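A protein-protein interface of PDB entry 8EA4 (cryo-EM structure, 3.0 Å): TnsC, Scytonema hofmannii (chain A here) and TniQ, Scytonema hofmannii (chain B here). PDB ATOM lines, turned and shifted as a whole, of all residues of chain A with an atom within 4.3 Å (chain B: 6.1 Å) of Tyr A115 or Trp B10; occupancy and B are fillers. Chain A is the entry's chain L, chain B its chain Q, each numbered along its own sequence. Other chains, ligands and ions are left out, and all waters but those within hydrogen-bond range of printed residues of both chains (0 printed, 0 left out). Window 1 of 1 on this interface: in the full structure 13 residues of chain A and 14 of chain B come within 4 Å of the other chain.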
ATOM      1  N   PRO A  86     -14.650   3.298  22.441  1.00  0.00           N
ATOM      2  CA  PRO A  86     -13.379   3.889  21.969  1.00  0.00           C
ATOM      3  C   PRO A  86     -12.286   2.869  21.577  1.00  0.00           C
ATOM      4  O   PRO A  86     -12.392   1.703  21.948  1.00  0.00           O
ATOM      5  CB  PRO A  86     -12.905   4.792  23.101  1.00  0.00           C
ATOM      6  CG  PRO A  86     -13.569   4.223  24.334  1.00  0.00           C
ATOM      7  CD  PRO A  86     -14.910   3.786  23.786  1.00  0.00           C
ATOM      8  N   PRO A  87     -11.229   3.268  20.838  1.00  0.00           N
ATOM      9  CA  PRO A  87     -10.292   2.353  20.172  1.00  0.00           C
ATOM     10  C   PRO A  87      -9.156   1.822  21.053  1.00  0.00           C
ATOM     11  O   PRO A  87      -8.755   2.489  21.993  1.00  0.00           O
ATOM     12  CB  PRO A  87      -9.687   3.171  19.037  1.00  0.00           C
ATOM     13  CG  PRO A  87      -9.668   4.574  19.620  1.00  0.00           C
ATOM     14  CD  PRO A  87     -10.952   4.630  20.430  1.00  0.00           C
ATOM     15  N   THR A 110      -3.452  13.847  23.721  1.00  0.00           N
ATOM     16  CA  THR A 110      -4.895  13.877  23.473  1.00  0.00           C
ATOM     17  C   THR A 110      -5.241  13.979  21.983  1.00  0.00           C
ATOM     18  O   THR A 110      -6.146  13.296  21.515  1.00  0.00           O
ATOM     19  CB  THR A 110      -5.492  15.047  24.251  1.00  0.00           C
ATOM     20  OG1 THR A 110      -5.211  14.904  25.617  1.00  0.00           O
ATOM     21  CG2 THR A 110      -6.998  15.133  24.167  1.00  0.00           C
ATOM     22  N   LEU A 113      -4.781  10.806  19.495  1.00  0.00           N
ATOM     23  CA  LEU A 113      -5.908   9.891  19.609  1.00  0.00           C
ATOM     24  C   LEU A 113      -7.219  10.450  19.045  1.00  0.00           C
ATOM     25  O   LEU A 113      -8.215   9.739  19.009  1.00  0.00           O
ATOM     26  CB  LEU A 113      -6.073   9.523  21.082  1.00  0.00           C
ATOM     27  CG  LEU A 113      -4.853   8.821  21.694  1.00  0.00           C
ATOM     28  CD1 LEU A 113      -5.102   8.597  23.174  1.00  0.00           C
ATOM     29  CD2 LEU A 113      -4.586   7.463  21.050  1.00  0.00           C
ATOM     30  N   LYS A 114      -7.258  11.719  18.641  1.00  0.00           N
ATOM     31  CA  LYS A 114      -8.475  12.415  18.204  1.00  0.00           C
ATOM     32  C   LYS A 114      -9.614  12.337  19.221  1.00  0.00           C
ATOM     33  O   LYS A 114     -10.777  12.162  18.877  1.00  0.00           O
ATOM     34  CB  LYS A 114      -8.863  11.983  16.783  1.00  0.00           C
ATOM     35  CG  LYS A 114      -7.824  12.464  15.769  1.00  0.00           C
ATOM     36  CD  LYS A 114      -8.220  12.116  14.334  1.00  0.00           C
ATOM     37  CE  LYS A 114      -7.336  12.820  13.305  1.00  0.00           C
ATOM     38  NZ  LYS A 114      -7.593  14.274  13.229  1.00  0.00           N
ATOM     39  N   TYR A 115      -9.293  12.509  20.496  1.00  0.00           N
ATOM     40  CA  TYR A 115     -10.299  12.745  21.532  1.00  0.00           C
ATOM     41  C   TYR A 115     -10.918  14.130  21.331  1.00  0.00           C
ATOM     42  O   TYR A 115     -10.187  15.098  21.143  1.00  0.00           O
ATOM     43  CB  TYR A 115      -9.626  12.620  22.895  1.00  0.00           C
ATOM     44  CG  TYR A 115     -10.555  12.645  24.084  1.00  0.00           C
ATOM     45  CD1 TYR A 115     -11.453  11.589  24.280  1.00  0.00           C
ATOM     46  CD2 TYR A 115     -10.460  13.666  25.035  1.00  0.00           C
ATOM     47  CE1 TYR A 115     -12.229  11.525  25.448  1.00  0.00           C
ATOM     48  CE2 TYR A 115     -11.233  13.602  26.204  1.00  0.00           C
ATOM     49  CZ  TYR A 115     -12.103  12.527  26.421  1.00  0.00           C
ATOM     50  OH  TYR A 115     -12.837  12.479  27.554  1.00  0.00           O
ATOM     51  N   ARG A 116     -12.248  14.262  21.311  1.00  0.00           N
ATOM     52  CA  ARG A 116     -12.895  15.501  20.844  1.00  0.00           C
ATOM     53  C   ARG A 116     -12.711  16.696  21.774  1.00  0.00           C
ATOM     54  O   ARG A 116     -12.699  17.825  21.292  1.00  0.00           O
ATOM     55  CB  ARG A 116     -14.390  15.294  20.576  1.00  0.00           C
ATOM     56  CG  ARG A 116     -14.688  14.436  19.341  1.00  0.00           C
ATOM     57  CD  ARG A 116     -16.196  14.250  19.114  1.00  0.00           C
ATOM     58  NE  ARG A 116     -16.885  15.535  18.919  1.00  0.00           N
ATOM     59  CZ  ARG A 116     -18.162  15.812  19.077  1.00  0.00           C
ATOM     60  NH1 ARG A 116     -19.061  14.911  19.325  1.00  0.00           N
ATOM     61  NH2 ARG A 116     -18.559  17.037  18.978  1.00  0.00           N
ATOM     62  N   VAL A 117     -12.576  16.503  23.085  1.00  0.00           N
ATOM     63  CA  VAL A 117     -12.482  17.637  24.024  1.00  0.00           C
ATOM     64  C   VAL A 117     -11.191  18.415  23.777  1.00  0.00           C
ATOM     65  O   VAL A 117     -10.121  17.825  23.734  1.00  0.00           O
ATOM     66  CB  VAL A 117     -12.538  17.218  25.498  1.00  0.00           C
ATOM     67  CG1 VAL A 117     -12.860  18.437  26.362  1.00  0.00           C
ATOM     68  CG2 VAL A 117     -13.602  16.167  25.785  1.00  0.00           C
ATOM     69  N   ARG A 128      -7.571  14.295  32.449  1.00  0.00           N
ATOM     70  CA  ARG A 128      -8.127  13.832  31.177  1.00  0.00           C
ATOM     71  C   ARG A 128      -7.139  13.002  30.358  1.00  0.00           C
ATOM     72  O   ARG A 128      -7.543  12.032  29.738  1.00  0.00           O
ATOM     73  CB  ARG A 128      -8.585  15.081  30.430  1.00  0.00           C
ATOM     74  CG  ARG A 128      -9.295  14.848  29.100  1.00  0.00           C
ATOM     75  CD  ARG A 128      -9.601  16.214  28.476  1.00  0.00           C
ATOM     76  NE  ARG A 128     -10.673  16.919  29.201  1.00  0.00           N
ATOM     77  CZ  ARG A 128     -10.933  18.208  29.155  1.00  0.00           C
ATOM     78  NH1 ARG A 128     -10.235  19.021  28.426  1.00  0.00           N
ATOM     79  NH2 ARG A 128     -11.909  18.704  29.839  1.00  0.00           N
ATOM     80  N   VAL A 132      -7.615   9.112  29.225  1.00  0.00           N
ATOM     81  CA  VAL A 132      -7.639   8.565  27.857  1.00  0.00           C
ATOM     82  C   VAL A 132      -6.523   7.574  27.593  1.00  0.00           C
ATOM     83  O   VAL A 132      -6.684   6.774  26.698  1.00  0.00           O
ATOM     84  CB  VAL A 132      -7.658   9.606  26.731  1.00  0.00           C
ATOM     85  CG1 VAL A 132      -8.890  10.502  26.811  1.00  0.00           C
ATOM     86  CG2 VAL A 132      -6.416  10.470  26.673  1.00  0.00           C
ATOM     87  N   VAL B   7      -8.070   6.812  12.986  1.00  0.00           N
ATOM     88  CA  VAL B   7      -9.015   6.836  14.108  1.00  0.00           C
ATOM     89  C   VAL B   7     -10.153   7.815  13.825  1.00  0.00           C
ATOM     90  O   VAL B   7      -9.943   8.829  13.194  1.00  0.00           O
ATOM     91  CB  VAL B   7      -8.282   7.243  15.398  1.00  0.00           C
ATOM     92  CG1 VAL B   7      -9.186   7.347  16.618  1.00  0.00           C
ATOM     93  CG2 VAL B   7      -7.158   6.275  15.741  1.00  0.00           C
ATOM     94  N   LYS B   8     -11.353   7.562  14.326  1.00  0.00           N
ATOM     95  CA  LYS B   8     -12.525   8.450  14.240  1.00  0.00           C
ATOM     96  C   LYS B   8     -12.665   9.304  15.505  1.00  0.00           C
ATOM     97  O   LYS B   8     -12.550   8.745  16.591  1.00  0.00           O
ATOM     98  CB  LYS B   8     -13.788   7.606  14.064  1.00  0.00           C
ATOM     99  CG  LYS B   8     -13.824   6.802  12.762  1.00  0.00           C
ATOM    100  CD  LYS B   8     -13.831   7.616  11.467  1.00  0.00           C
ATOM    101  CE  LYS B   8     -15.018   8.564  11.393  1.00  0.00           C
ATOM    102  NZ  LYS B   8     -15.177   9.147  10.064  1.00  0.00           N
ATOM    103  N   PRO B   9     -12.936  10.618  15.420  1.00  0.00           N
ATOM    104  CA  PRO B   9     -13.016  11.474  16.596  1.00  0.00           C
ATOM    105  C   PRO B   9     -14.040  10.986  17.611  1.00  0.00           C
ATOM    106  O   PRO B   9     -15.145  10.619  17.233  1.00  0.00           O
ATOM    107  CB  PRO B   9     -13.373  12.864  16.092  1.00  0.00           C
ATOM    108  CG  PRO B   9     -12.864  12.860  14.660  1.00  0.00           C
ATOM    109  CD  PRO B   9     -13.048  11.419  14.219  1.00  0.00           C
ATOM    110  N   TRP B  10     -13.698  10.983  18.892  1.00  0.00           N
ATOM    111  CA  TRP B  10     -14.485  10.267  19.896  1.00  0.00           C
ATOM    112  C   TRP B  10     -14.480  10.909  21.278  1.00  0.00           C
ATOM    113  O   TRP B  10     -13.712  11.821  21.557  1.00  0.00           O
ATOM    114  CB  TRP B  10     -13.951   8.842  19.968  1.00  0.00           C
ATOM    115  CG  TRP B  10     -12.574   8.744  20.520  1.00  0.00           C
ATOM    116  CD1 TRP B  10     -11.447   8.918  19.814  1.00  0.00           C
ATOM    117  CD2 TRP B  10     -12.148   8.546  21.896  1.00  0.00           C
ATOM    118  NE1 TRP B  10     -10.362   8.809  20.646  1.00  0.00           N
ATOM    119  CE2 TRP B  10     -10.732   8.549  21.940  1.00  0.00           C
ATOM    120  CE3 TRP B  10     -12.816   8.347  23.109  1.00  0.00           C
ATOM    121  CZ2 TRP B  10     -10.012   8.344  23.117  1.00  0.00           C
ATOM    122  CZ3 TRP B  10     -12.108   8.153  24.305  1.00  0.00           C
ATOM    123  CH2 TRP B  10     -10.709   8.144  24.307  1.00  0.00           C
ATOM    124  N   LEU B  11     -15.367  10.415  22.132  1.00  0.00           N
ATOM    125  CA  LEU B  11     -15.535  10.739  23.546  1.00  0.00           C
ATOM    126  C   LEU B  11     -15.901   9.470  24.302  1.00  0.00           C
ATOM    127  O   LEU B  11     -16.335   8.500  23.691  1.00  0.00           O
ATOM    128  CB  LEU B  11     -16.670  11.750  23.719  1.00  0.00           C
ATOM    129  CG  LEU B  11     -16.340  13.126  23.170  1.00  0.00           C
ATOM    130  CD1 LEU B  11     -17.547  14.040  23.274  1.00  0.00           C
ATOM    131  CD2 LEU B  11     -15.195  13.756  23.956  1.00  0.00           C
ATOM    132  N   PHE B  12     -15.784   9.447  25.622  1.00  0.00           N
ATOM    133  CA  PHE B  12     -16.424   8.397  26.404  1.00  0.00           C
ATOM    134  C   PHE B  12     -17.934   8.647  26.415  1.00  0.00           C
ATOM    135  O   PHE B  12     -18.460   9.247  27.344  1.00  0.00           O
ATOM    136  CB  PHE B  12     -15.834   8.351  27.812  1.00  0.00           C
ATOM    137  CG  PHE B  12     -14.392   7.900  27.876  1.00  0.00           C
ATOM    138  CD1 PHE B  12     -13.366   8.811  28.175  1.00  0.00           C
ATOM    139  CD2 PHE B  12     -14.082   6.550  27.684  1.00  0.00           C
ATOM    140  CE1 PHE B  12     -12.038   8.371  28.277  1.00  0.00           C
ATOM    141  CE2 PHE B  12     -12.754   6.110  27.782  1.00  0.00           C
ATOM    142  CZ  PHE B  12     -11.730   7.020  28.077  1.00  0.00           C
ATOM    143  N   LEU B  13     -18.642   8.254  25.356  1.00  0.00           N
ATOM    144  CA  LEU B  13     -20.107   8.273  25.340  1.00  0.00           C
ATOM    145  C   LEU B  13     -20.678   7.329  26.397  1.00  0.00           C
ATOM    146  O   LEU B  13     -20.060   6.321  26.739  1.00  0.00           O
ATOM    147  CB  LEU B  13     -20.672   7.859  23.966  1.00  0.00           C
ATOM    148  CG  LEU B  13     -20.578   8.863  22.809  1.00  0.00           C
ATOM    149  CD1 LEU B  13     -20.925  10.277  23.263  1.00  0.00           C
ATOM    150  CD2 LEU B  13     -19.216   8.888  22.133  1.00  0.00           C
ATOM    151  N   ALA B  32     -17.632  10.206  32.915  1.00  0.00           N
ATOM    152  CA  ALA B  32     -17.125   9.344  31.852  1.00  0.00           C
ATOM    153  C   ALA B  32     -16.028  10.047  31.042  1.00  0.00           C
ATOM    154  O   ALA B  32     -14.982   9.460  30.782  1.00  0.00           O
ATOM    155  CB  ALA B  32     -18.305   8.945  30.969  1.00  0.00           C
ATOM    156  N   ASN B  33     -16.246  11.320  30.721  1.00  0.00           N
ATOM    157  CA  ASN B  33     -15.211  12.265  30.325  1.00  0.00           C
ATOM    158  C   ASN B  33     -14.943  13.153  31.527  1.00  0.00           C
ATOM    159  O   ASN B  33     -15.904  13.570  32.171  1.00  0.00           O
ATOM    160  CB  ASN B  33     -15.710  13.115  29.157  1.00  0.00           C
ATOM    161  CG  ASN B  33     -16.192  12.231  28.038  1.00  0.00           C
ATOM    162  OD1 ASN B  33     -15.409  11.716  27.259  1.00  0.00           O
ATOM    163  ND2 ASN B  33     -17.476  11.987  27.971  1.00  0.00           N
ATOM    164  N   HIS B  34     -13.703  13.511  31.834  1.00  0.00           N
ATOM    165  CA  HIS B  34     -13.457  14.380  32.994  1.00  0.00           C
ATOM    166  C   HIS B  34     -13.669  15.842  32.611  1.00  0.00           C
ATOM    167  O   HIS B  34     -12.745  16.505  32.150  1.00  0.00           O
ATOM    168  CB  HIS B  34     -12.069  14.133  33.595  1.00  0.00           C
ATOM    169  CG  HIS B  34     -11.896  12.810  34.293  1.00  0.00           C
ATOM    170  ND1 HIS B  34     -10.876  12.536  35.204  1.00  0.00           N
ATOM    171  CD2 HIS B  34     -12.646  11.684  34.136  1.00  0.00           C
ATOM    172  CE1 HIS B  34     -11.047  11.260  35.582  1.00  0.00           C
ATOM    173  NE2 HIS B  34     -12.098  10.723  34.947  1.00  0.00           N
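The backbone carbonyl oxygen (O) of Leu A113 lies within hydrogen-bond range of the indole nitrogen (NE1) of Trp B10. The backbone carbonyl oxygen of Lys A114 sits at hydrogen-bond distance from the backbone NH of Trp B10 (3.2 Å). The side-chain hydroxyl (OH) of Tyr A115 is in hydrogen-bond range of the side-chain amide oxygen (OD1) of Asn B33 (2.7 Å). The backbone NH of Arg A116 lies within hydrogen-bond range of the backbone carbonyl oxygen of Trp B10 (2.9 Å). The guanidinium group (NH2) of Arg A128 is in hydrogen-bond range of the backbone carbonyl oxygen (O) of His B34, 3.3 Å away.
N of Tyr A115 lies within hydrogen-bond range of O of Thr A110 (3.4 Å). N of Phe B12 sits at hydrogen-bond distance from OD1 of Asn B33 (2.8 Å).
Pro A86 touches Trp B10 (CB to CE3, 3.6 Å). Val B7 touches Leu A113. Val B7 touches Lys A114 (O to CD, 3.9 Å). Tyr A115 touches Trp B10. Leu B11 touches Tyr A115. Phe B12 touches Tyr A115. Pro B9 touches Arg A116. CB of Arg A116 touches CD2 of Leu B11, 3.8 Å away. Leu B11 touches Val A117. Trp B10 touches Val A132 (CH2 to CG1, 3.9 Å).
Tyr A115 touches four residues of chain B. Of chain A, only Pro A86 (3.6 Å), Leu A113 (2.9 Å), Lys A114 (3.2 Å), Tyr A115 (3.5 Å), Arg A116 (2.9 Å) and Val A132 (3.9 Å) come within 4 Å of Trp B10. Of the printed residues of chain B, Leu A113 touches Val B7 and Trp B10. Of the printed residues of chain A, His B34 touches Arg A128 (3.3 Å). Of the printed residues of chain B, Pro A86 touches Trp B10 (3.6 Å). The nearest residue of chain B that does not touch Tyr A115 is His B34 (4.5 Å).
Hydrophobic or aromatic side chains of chain B that line the printed part of chain A: Val B7, Pro B9, Trp B10, Leu B11 and Phe B12. Hydrophobic or aromatic side chains of chain A that line the printed part of chain B: Pro A86, Tyr A115, Val A117 and Val A132. Among the printed residues, 16 pairs touch across the chains. Among the printed residues, no Asp or Glu carboxylate lies within 4 Å of a Lys or Arg side-chain nitrogen of the other chain.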
